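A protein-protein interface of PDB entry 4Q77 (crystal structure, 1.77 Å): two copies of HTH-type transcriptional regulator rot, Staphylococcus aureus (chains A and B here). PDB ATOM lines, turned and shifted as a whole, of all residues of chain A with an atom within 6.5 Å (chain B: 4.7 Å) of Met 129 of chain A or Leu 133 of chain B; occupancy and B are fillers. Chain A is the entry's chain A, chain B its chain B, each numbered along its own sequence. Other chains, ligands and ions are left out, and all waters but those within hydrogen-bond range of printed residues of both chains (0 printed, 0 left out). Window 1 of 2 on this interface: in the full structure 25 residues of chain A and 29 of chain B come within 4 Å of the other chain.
The side-chain amide nitrogen (NE2) of Gln 130 of chain A is in hydrogen-bond range of the side-chain amide oxygen (OE1) of Gln 130 of chain B (3.0 Å).
The side-chain amide nitrogen of Gln 130 of chain B is in hydrogen-bond range of the side-chain amide oxygen of Asn 134 of chain B, 2.8 Å away. OD1 of Asn 134 of chain A sits at hydrogen-bond distance from NE2 of Gln 130 of chain A, 2.8 Å away.
CD1 of Ile 28 of chain A touches CG of Leu 24 of chain B, 3.8 Å away. Ile 136 of chain B touches Ile 122 of chain A (O to CG2, 3.4 Å). CD1 of Ile 137 of chain B touches O of Ala 126 of chain A, at 3.8 Å. Met 129 of chain A touches Leu 133 of chain B (O to CD2, 3.8 Å). OE1 of Gln 130 of chain A touches CD2 of Leu 133 of chain B, 3.6 Å away. Met 129 of chain B touches Leu 133 of chain A. OE1 of Gln 130 of chain B touches CD2 of Leu 133 of chain A, at 3.7 Å. CD2 of Leu 133 of chain A touches CD2 of Leu 133 of chain B (3.7 Å).
Of chain B, only Leu 133 comes within 4 Å of Met 129 of chain A. Leu 133 of chain B touches just these residues of chain A: Met 129 (3.8 Å), Gln 130 (3.6 Å) and Leu 133 (3.7 Å). Printed residues of chain B within 4 Å of Ile 28 of chain A: Leu 24 (3.8 Å). Of the printed residues of chain A, Ile 136 of chain B touches Ile 122 (3.4 Å). Of the printed residues of chain A, Met 129 of chain B touches Leu 133 (3.7 Å). Printed residues of chain B within 4 Å of Leu 133 of chain A: Met 129 (3.7 Å), Gln 130 (3.7 Å) and Leu 133 (3.7 Å). Asn 134 of chain A touches none of the printed residues of chain B. Thr 127 of chain A touches none of the printed residues of chain B. The nearest residue of chain B that does not touch Met 129 of chain A is Ile 136 of chain B (4.3 Å).
Of the 18 printed residues of chain A, 6 touch a printed residue of chain B. Printed residues of chain A that touch a printed residue of chain B: Ile 28, Ile 122, Ala 126, Met 129, Gln 130 and Leu 133. Hydrophobic or aromatic side chains of chain A that line the printed part of chain B: Ile 28, Ile 122 and Leu 133. Among the printed residues, 9 pairs touch across the chains. Among the printed residues, no Asp or Glu carboxylate lies within 4 Å of a Lys or Arg side-chain nitrogen of the other chain.
Met 129 of chain A touches Leu 133 of chain B, and with the chains exchanged Leu 133 of chain A touches Met 129 of chain B. Gln 130 of chain A touches its own counterpart, Gln 130 of chain B. Gln 130 of chain A touches Leu 133 of chain B, and with the chains exchanged Leu 133 of chain A touches Gln 130 of chain B. Leu 133 of chain B touches its own counterpart, Leu 133 of chain A. Positions printed for both chains: 24, 129, 130, 131, 132, 133, 134 and 136. Of the 9 pairs that touch across the chains among the printed residues, 6 have their exchanged pair printed and touching as well.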
ATOM      1  N   LEU A  24     -20.931 -21.813 -20.953  1.00  0.00           N
ATOM      2  CA  LEU A  24     -20.185 -20.784 -20.234  1.00  0.00           C
ATOM      3  C   LEU A  24     -20.036 -21.099 -18.741  1.00  0.00           C
ATOM      4  O   LEU A  24     -18.945 -20.936 -18.164  1.00  0.00           O
ATOM      5  CB  LEU A  24     -20.842 -19.411 -20.428  1.00  0.00           C
ATOM      6  CG  LEU A  24     -20.114 -18.179 -19.854  1.00  0.00           C
ATOM      7  CD1 LEU A  24     -18.660 -18.100 -20.323  1.00  0.00           C
ATOM      8  CD2 LEU A  24     -20.845 -16.890 -20.197  1.00  0.00           C
ATOM      9  N   ASP A  27     -17.359 -23.702 -18.457  1.00  0.00           N
ATOM     10  CA  ASP A  27     -16.028 -23.076 -18.612  1.00  0.00           C
ATOM     11  C   ASP A  27     -15.540 -22.473 -17.279  1.00  0.00           C
ATOM     12  O   ASP A  27     -14.394 -22.651 -16.871  1.00  0.00           O
ATOM     13  CB  ASP A  27     -16.052 -21.930 -19.648  1.00  0.00           C
ATOM     14  CG  ASP A  27     -16.276 -22.393 -21.094  1.00  0.00           C
ATOM     15  OD1 ASP A  27     -15.908 -23.519 -21.470  1.00  0.00           O
ATOM     16  OD2 ASP A  27     -16.813 -21.569 -21.881  1.00  0.00           O
ATOM     17  N   ILE A  28     -16.419 -21.738 -16.603  1.00  0.00           N
ATOM     18  CA  ILE A  28     -16.077 -21.117 -15.334  1.00  0.00           C
ATOM     19  C   ILE A  28     -15.741 -22.169 -14.277  1.00  0.00           C
ATOM     20  O   ILE A  28     -14.727 -22.065 -13.602  1.00  0.00           O
ATOM     21  CB  ILE A  28     -17.208 -20.176 -14.838  1.00  0.00           C
ATOM     22  CG1 ILE A  28     -17.366 -19.000 -15.809  1.00  0.00           C
ATOM     23  CG2 ILE A  28     -16.922 -19.661 -13.436  1.00  0.00           C
ATOM     24  CD1 ILE A  28     -18.631 -18.192 -15.582  1.00  0.00           C
ATOM     25  N   ILE A  31     -12.328 -23.741 -14.954  1.00  0.00           N
ATOM     26  CA  ILE A  31     -11.238 -22.902 -14.478  1.00  0.00           C
ATOM     27  C   ILE A  31     -11.032 -23.115 -12.999  1.00  0.00           C
ATOM     28  O   ILE A  31      -9.900 -23.320 -12.562  1.00  0.00           O
ATOM     29  CB  ILE A  31     -11.476 -21.409 -14.771  1.00  0.00           C
ATOM     30  CG1 ILE A  31     -11.351 -21.179 -16.283  1.00  0.00           C
ATOM     31  CG2 ILE A  31     -10.502 -20.548 -13.967  1.00  0.00           C
ATOM     32  CD1 ILE A  31     -11.968 -19.898 -16.806  1.00  0.00           C
ATOM     33  N   ALA A 121      -5.098 -20.063 -17.113  1.00  0.00           N
ATOM     34  CA  ALA A 121      -6.275 -20.916 -17.231  1.00  0.00           C
ATOM     35  C   ALA A 121      -7.414 -20.137 -17.904  1.00  0.00           C
ATOM     36  O   ALA A 121      -8.108 -20.647 -18.778  1.00  0.00           O
ATOM     37  CB  ALA A 121      -6.690 -21.437 -15.866  1.00  0.00           C
ATOM     38  N   ILE A 122      -7.558 -18.875 -17.546  1.00  0.00           N
ATOM     39  CA  ILE A 122      -8.524 -18.002 -18.225  1.00  0.00           C
ATOM     40  C   ILE A 122      -8.179 -17.836 -19.698  1.00  0.00           C
ATOM     41  O   ILE A 122      -9.021 -18.079 -20.560  1.00  0.00           O
ATOM     42  CB  ILE A 122      -8.595 -16.635 -17.537  1.00  0.00           C
ATOM     43  CG1 ILE A 122      -9.218 -16.808 -16.137  1.00  0.00           C
ATOM     44  CG2 ILE A 122      -9.407 -15.641 -18.365  1.00  0.00           C
ATOM     45  CD1 ILE A 122      -9.059 -15.600 -15.248  1.00  0.00           C
ATOM     46  N   ALA A 123      -6.934 -17.457 -19.992  1.00  0.00           N
ATOM     47  CA  ALA A 123      -6.522 -17.193 -21.372  1.00  0.00           C
ATOM     48  C   ALA A 123      -6.744 -18.404 -22.279  1.00  0.00           C
ATOM     49  O   ALA A 123      -7.066 -18.258 -23.461  1.00  0.00           O
ATOM     50  CB  ALA A 123      -5.070 -16.756 -21.414  1.00  0.00           C
ATOM     51  N   ARG A 125      -9.172 -20.384 -22.253  1.00  0.00           N
ATOM     52  CA  ARG A 125     -10.573 -20.524 -22.599  1.00  0.00           C
ATOM     53  C   ARG A 125     -11.221 -19.205 -23.052  1.00  0.00           C
ATOM     54  O   ARG A 125     -12.408 -19.188 -23.356  1.00  0.00           O
ATOM     55  CB  ARG A 125     -11.336 -21.070 -21.395  1.00  0.00           C
ATOM     56  CG  ARG A 125     -11.067 -22.520 -21.075  1.00  0.00           C
ATOM     57  CD  ARG A 125     -11.626 -22.889 -19.720  1.00  0.00           C
ATOM     58  NE  ARG A 125     -11.266 -24.262 -19.379  1.00  0.00           N
ATOM     59  CZ  ARG A 125     -11.963 -25.354 -19.704  1.00  0.00           C
ATOM     60  NH1 ARG A 125     -13.112 -25.286 -20.372  1.00  0.00           N
ATOM     61  NH2 ARG A 125     -11.499 -26.542 -19.343  1.00  0.00           N
ATOM     62  N   ALA A 126     -10.447 -18.130 -23.131  1.00  0.00           N
ATOM     63  CA  ALA A 126     -11.001 -16.782 -23.346  1.00  0.00           C
ATOM     64  C   ALA A 126     -11.817 -16.650 -24.636  1.00  0.00           C
ATOM     65  O   ALA A 126     -12.913 -16.095 -24.632  1.00  0.00           O
ATOM     66  CB  ALA A 126      -9.888 -15.737 -23.303  1.00  0.00           C
ATOM     67  N   THR A 127     -11.296 -17.159 -25.737  1.00  0.00           N
ATOM     68  CA  THR A 127     -12.003 -17.087 -27.009  1.00  0.00           C
ATOM     69  C   THR A 127     -13.353 -17.810 -26.965  1.00  0.00           C
ATOM     70  O   THR A 127     -14.367 -17.271 -27.405  1.00  0.00           O
ATOM     71  CB  THR A 127     -11.133 -17.668 -28.132  1.00  0.00           C
ATOM     72  OG1 THR A 127      -9.990 -16.828 -28.285  1.00  0.00           O
ATOM     73  CG2 THR A 127     -11.884 -17.733 -29.443  1.00  0.00           C
ATOM     74  N   ALA A 128     -13.346 -19.031 -26.440  1.00  0.00           N
ATOM     75  CA  ALA A 128     -14.550 -19.843 -26.341  1.00  0.00           C
ATOM     76  C   ALA A 128     -15.552 -19.147 -25.435  1.00  0.00           C
ATOM     77  O   ALA A 128     -16.740 -19.137 -25.717  1.00  0.00           O
ATOM     78  CB  ALA A 128     -14.221 -21.229 -25.809  1.00  0.00           C
ATOM     79  N   MET A 129     -15.079 -18.569 -24.342  1.00  0.00           N
ATOM     80  CA  MET A 129     -15.990 -17.915 -23.389  1.00  0.00           C
ATOM     81  C   MET A 129     -16.686 -16.704 -24.011  1.00  0.00           C
ATOM     82  O   MET A 129     -17.922 -16.526 -23.863  1.00  0.00           O
ATOM     83  CB  MET A 129     -15.252 -17.528 -22.102  1.00  0.00           C
ATOM     84  CG  MET A 129     -14.913 -18.730 -21.226  1.00  0.00           C
ATOM     85  SD  MET A 129     -14.303 -18.306 -19.582  1.00  0.00           S
ATOM     86  CE  MET A 129     -12.853 -17.365 -19.956  1.00  0.00           C
ATOM     87  N   GLN A 130     -15.927 -15.893 -24.736  1.00  0.00           N
ATOM     88  CA  GLN A 130     -16.520 -14.744 -25.408  1.00  0.00           C
ATOM     89  C   GLN A 130     -17.476 -15.187 -26.519  1.00  0.00           C
ATOM     90  O   GLN A 130     -18.535 -14.582 -26.716  1.00  0.00           O
ATOM     91  CB  GLN A 130     -15.443 -13.811 -25.953  1.00  0.00           C
ATOM     92  CG  GLN A 130     -15.996 -12.538 -26.579  1.00  0.00           C
ATOM     93  CD  GLN A 130     -16.740 -11.674 -25.577  1.00  0.00           C
ATOM     94  OE1 GLN A 130     -16.136 -11.120 -24.659  1.00  0.00           O
ATOM     95  NE2 GLN A 130     -18.056 -11.560 -25.738  1.00  0.00           N
ATOM     96  N   ASN A 131     -17.120 -16.239 -27.243  1.00  0.00           N
ATOM     97  CA  ASN A 131     -18.016 -16.783 -28.259  1.00  0.00           C
ATOM     98  C   ASN A 131     -19.310 -17.268 -27.625  1.00  0.00           C
ATOM     99  O   ASN A 131     -20.385 -17.047 -28.186  1.00  0.00           O
ATOM    100  CB  ASN A 131     -17.360 -17.928 -29.034  1.00  0.00           C
ATOM    101  CG  ASN A 131     -16.270 -17.454 -29.984  1.00  0.00           C
ATOM    102  OD1 ASN A 131     -16.173 -16.274 -30.319  1.00  0.00           O
ATOM    103  ND2 ASN A 131     -15.455 -18.395 -30.452  1.00  0.00           N
ATOM    104  N   SER A 132     -19.215 -17.927 -26.471  1.00  0.00           N
ATOM    105  CA  SER A 132     -20.429 -18.355 -25.762  1.00  0.00           C
ATOM    106  C   SER A 132     -21.285 -17.154 -25.361  1.00  0.00           C
ATOM    107  O   SER A 132     -22.485 -17.146 -25.620  1.00  0.00           O
ATOM    108  CB  SER A 132     -20.112 -19.217 -24.549  1.00  0.00           C
ATOM    109  OG  SER A 132     -19.675 -20.510 -24.948  1.00  0.00           O
ATOM    110  N   LEU A 133     -20.674 -16.145 -24.749  1.00  0.00           N
ATOM    111  CA  LEU A 133     -21.427 -14.978 -24.312  1.00  0.00           C
ATOM    112  C   LEU A 133     -22.025 -14.221 -25.475  1.00  0.00           C
ATOM    113  O   LEU A 133     -23.134 -13.711 -25.350  1.00  0.00           O
ATOM    114  CB  LEU A 133     -20.600 -14.046 -23.432  1.00  0.00           C
ATOM    115  CG  LEU A 133     -21.405 -12.972 -22.674  1.00  0.00           C
ATOM    116  CD1 LEU A 133     -22.471 -13.612 -21.794  1.00  0.00           C
ATOM    117  CD2 LEU A 133     -20.507 -12.063 -21.840  1.00  0.00           C
ATOM    118  N   ASN A 134     -21.338 -14.169 -26.615  1.00  0.00           N
ATOM    119  CA  ASN A 134     -21.938 -13.527 -27.784  1.00  0.00           C
ATOM    120  C   ASN A 134     -23.221 -14.262 -28.202  1.00  0.00           C
ATOM    121  O   ASN A 134     -24.226 -13.634 -28.564  1.00  0.00           O
ATOM    122  CB  ASN A 134     -20.954 -13.462 -28.955  1.00  0.00           C
ATOM    123  CG  ASN A 134     -19.796 -12.491 -28.718  1.00  0.00           C
ATOM    124  OD1 ASN A 134     -19.857 -11.584 -27.879  1.00  0.00           O
ATOM    125  ND2 ASN A 134     -18.733 -12.680 -29.470  1.00  0.00           N
ATOM    126  N   ILE A 136     -25.165 -16.126 -26.264  1.00  0.00           N
ATOM    127  CA  ILE A 136     -26.127 -15.897 -25.173  1.00  0.00           C
ATOM    128  C   ILE A 136     -26.820 -14.545 -25.363  1.00  0.00           C
ATOM    129  O   ILE A 136     -28.059 -14.438 -25.367  1.00  0.00           O
ATOM    130  CB  ILE A 136     -25.406 -15.949 -23.798  1.00  0.00           C
ATOM    131  CG1 ILE A 136     -25.005 -17.389 -23.447  1.00  0.00           C
ATOM    132  CG2 ILE A 136     -26.267 -15.375 -22.680  1.00  0.00           C
ATOM    133  CD1 ILE A 136     -23.903 -17.482 -22.399  1.00  0.00           C
ATOM    134  N   LEU B  24     -20.027 -13.528 -12.734  1.00  0.00           N
ATOM    135  CA  LEU B  24     -20.605 -14.057 -13.958  1.00  0.00           C
ATOM    136  C   LEU B  24     -21.350 -15.364 -13.700  1.00  0.00           C
ATOM    137  O   LEU B  24     -22.462 -15.551 -14.190  1.00  0.00           O
ATOM    138  CB  LEU B  24     -19.497 -14.239 -15.012  1.00  0.00           C
ATOM    139  CG  LEU B  24     -19.914 -14.716 -16.401  1.00  0.00           C
ATOM    140  CD1 LEU B  24     -21.018 -13.839 -16.999  1.00  0.00           C
ATOM    141  CD2 LEU B  24     -18.714 -14.799 -17.346  1.00  0.00           C
ATOM    142  N   MET B 129     -23.085  -8.967 -17.610  1.00  0.00           N
ATOM    143  CA  MET B 129     -22.336 -10.194 -17.940  1.00  0.00           C
ATOM    144  C   MET B 129     -21.143  -9.885 -18.830  1.00  0.00           C
ATOM    145  O   MET B 129     -20.034 -10.402 -18.587  1.00  0.00           O
ATOM    146  CB  MET B 129     -23.247 -11.245 -18.573  1.00  0.00           C
ATOM    147  CG  MET B 129     -24.236 -11.857 -17.569  1.00  0.00           C
ATOM    148  SD  MET B 129     -25.130 -13.294 -18.198  1.00  0.00           S
ATOM    149  CE  MET B 129     -26.128 -12.558 -19.478  1.00  0.00           C
ATOM    150  N   GLN B 130     -21.337  -9.006 -19.815  1.00  0.00           N
ATOM    151  CA  GLN B 130     -20.212  -8.594 -20.671  1.00  0.00           C
ATOM    152  C   GLN B 130     -19.168  -7.823 -19.884  1.00  0.00           C
ATOM    153  O   GLN B 130     -17.973  -7.988 -20.133  1.00  0.00           O
ATOM    154  CB  GLN B 130     -20.660  -7.775 -21.886  1.00  0.00           C
ATOM    155  CG  GLN B 130     -19.523  -7.461 -22.860  1.00  0.00           C
ATOM    156  CD  GLN B 130     -18.909  -8.712 -23.482  1.00  0.00           C
ATOM    157  OE1 GLN B 130     -19.567  -9.438 -24.222  1.00  0.00           O
ATOM    158  NE2 GLN B 130     -17.642  -8.959 -23.192  1.00  0.00           N
ATOM    159  N   ASN B 131     -19.602  -6.977 -18.951  1.00  0.00           N
ATOM    160  CA  ASN B 131     -18.667  -6.256 -18.084  1.00  0.00           C
ATOM    161  C   ASN B 131     -17.811  -7.208 -17.241  1.00  0.00           C
ATOM    162  O   ASN B 131     -16.594  -7.004 -17.093  1.00  0.00           O
ATOM    163  CB  ASN B 131     -19.396  -5.279 -17.159  1.00  0.00           C
ATOM    164  CG  ASN B 131     -19.926  -4.047 -17.882  1.00  0.00           C
ATOM    165  OD1 ASN B 131     -19.575  -3.769 -19.024  1.00  0.00           O
ATOM    166  ND2 ASN B 131     -20.767  -3.285 -17.192  1.00  0.00           N
ATOM    167  N   SER B 132     -18.444  -8.238 -16.686  1.00  0.00           N
ATOM    168  CA  SER B 132     -17.732  -9.219 -15.891  1.00  0.00           C
ATOM    169  C   SER B 132     -16.739  -9.954 -16.766  1.00  0.00           C
ATOM    170  O   SER B 132     -15.591 -10.110 -16.385  1.00  0.00           O
ATOM    171  CB  SER B 132     -18.684 -10.228 -15.244  1.00  0.00           C
ATOM    172  OG  SER B 132     -19.430  -9.632 -14.201  1.00  0.00           O
ATOM    173  N   LEU B 133     -17.181 -10.404 -17.936  1.00  0.00           N
ATOM    174  CA  LEU B 133     -16.287 -11.145 -18.823  1.00  0.00           C
ATOM    175  C   LEU B 133     -15.127 -10.292 -19.337  1.00  0.00           C
ATOM    176  O   LEU B 133     -14.017 -10.806 -19.470  1.00  0.00           O
ATOM    177  CB  LEU B 133     -17.034 -11.792 -19.992  1.00  0.00           C
ATOM    178  CG  LEU B 133     -16.193 -12.821 -20.771  1.00  0.00           C
ATOM    179  CD1 LEU B 133     -15.734 -13.991 -19.897  1.00  0.00           C
ATOM    180  CD2 LEU B 133     -16.982 -13.337 -21.950  1.00  0.00           C
ATOM    181  N   ASN B 134     -15.351  -9.008 -19.613  1.00  0.00           N
ATOM    182  CA  ASN B 134     -14.232  -8.125 -19.962  1.00  0.00           C
ATOM    183  C   ASN B 134     -13.160  -8.143 -18.874  1.00  0.00           C
ATOM    184  O   ASN B 134     -11.960  -8.226 -19.170  1.00  0.00           O
ATOM    185  CB  ASN B 134     -14.695  -6.679 -20.175  1.00  0.00           C
ATOM    186  CG  ASN B 134     -15.471  -6.489 -21.462  1.00  0.00           C
ATOM    187  OD1 ASN B 134     -15.464  -7.340 -22.352  1.00  0.00           O
ATOM    188  ND2 ASN B 134     -16.140  -5.358 -21.572  1.00  0.00           N
ATOM    189  N   ALA B 135     -13.597  -8.063 -17.617  1.00  0.00           N
ATOM    190  CA  ALA B 135     -12.676  -8.073 -16.480  1.00  0.00           C
ATOM    191  C   ALA B 135     -11.939  -9.405 -16.376  1.00  0.00           C
ATOM    192  O   ALA B 135     -10.718  -9.441 -16.182  1.00  0.00           O
ATOM    193  CB  ALA B 135     -13.421  -7.787 -15.188  1.00  0.00           C
ATOM    194  N   ILE B 136     -12.685 -10.491 -16.518  1.00  0.00           N
ATOM    195  CA  ILE B 136     -12.118 -11.844 -16.487  1.00  0.00           C
ATOM    196  C   ILE B 136     -11.017 -12.015 -17.533  1.00  0.00           C
ATOM    197  O   ILE B 136      -9.915 -12.464 -17.223  1.00  0.00           O
ATOM    198  CB  ILE B 136     -13.217 -12.902 -16.697  1.00  0.00           C
ATOM    199  CG1 ILE B 136     -14.133 -12.947 -15.477  1.00  0.00           C
ATOM    200  CG2 ILE B 136     -12.619 -14.291 -16.920  1.00  0.00           C
ATOM    201  CD1 ILE B 136     -15.488 -13.544 -15.773  1.00  0.00           C
ATOM    202  N   ILE B 137     -11.321 -11.633 -18.761  1.00  0.00           N
ATOM    203  CA  ILE B 137     -10.437 -11.881 -19.896  1.00  0.00           C
ATOM    204  C   ILE B 137      -9.209 -10.981 -19.845  1.00  0.00           C
ATOM    205  O   ILE B 137      -8.162 -11.336 -20.385  1.00  0.00           O
ATOM    206  CB  ILE B 137     -11.205 -11.762 -21.231  1.00  0.00           C
ATOM    207  CG1 ILE B 137     -12.127 -12.976 -21.376  1.00  0.00           C
ATOM    208  CG2 ILE B 137     -10.257 -11.678 -22.420  1.00  0.00           C
ATOM    209  CD1 ILE B 137     -13.038 -12.945 -22.583  1.00  0.00           C
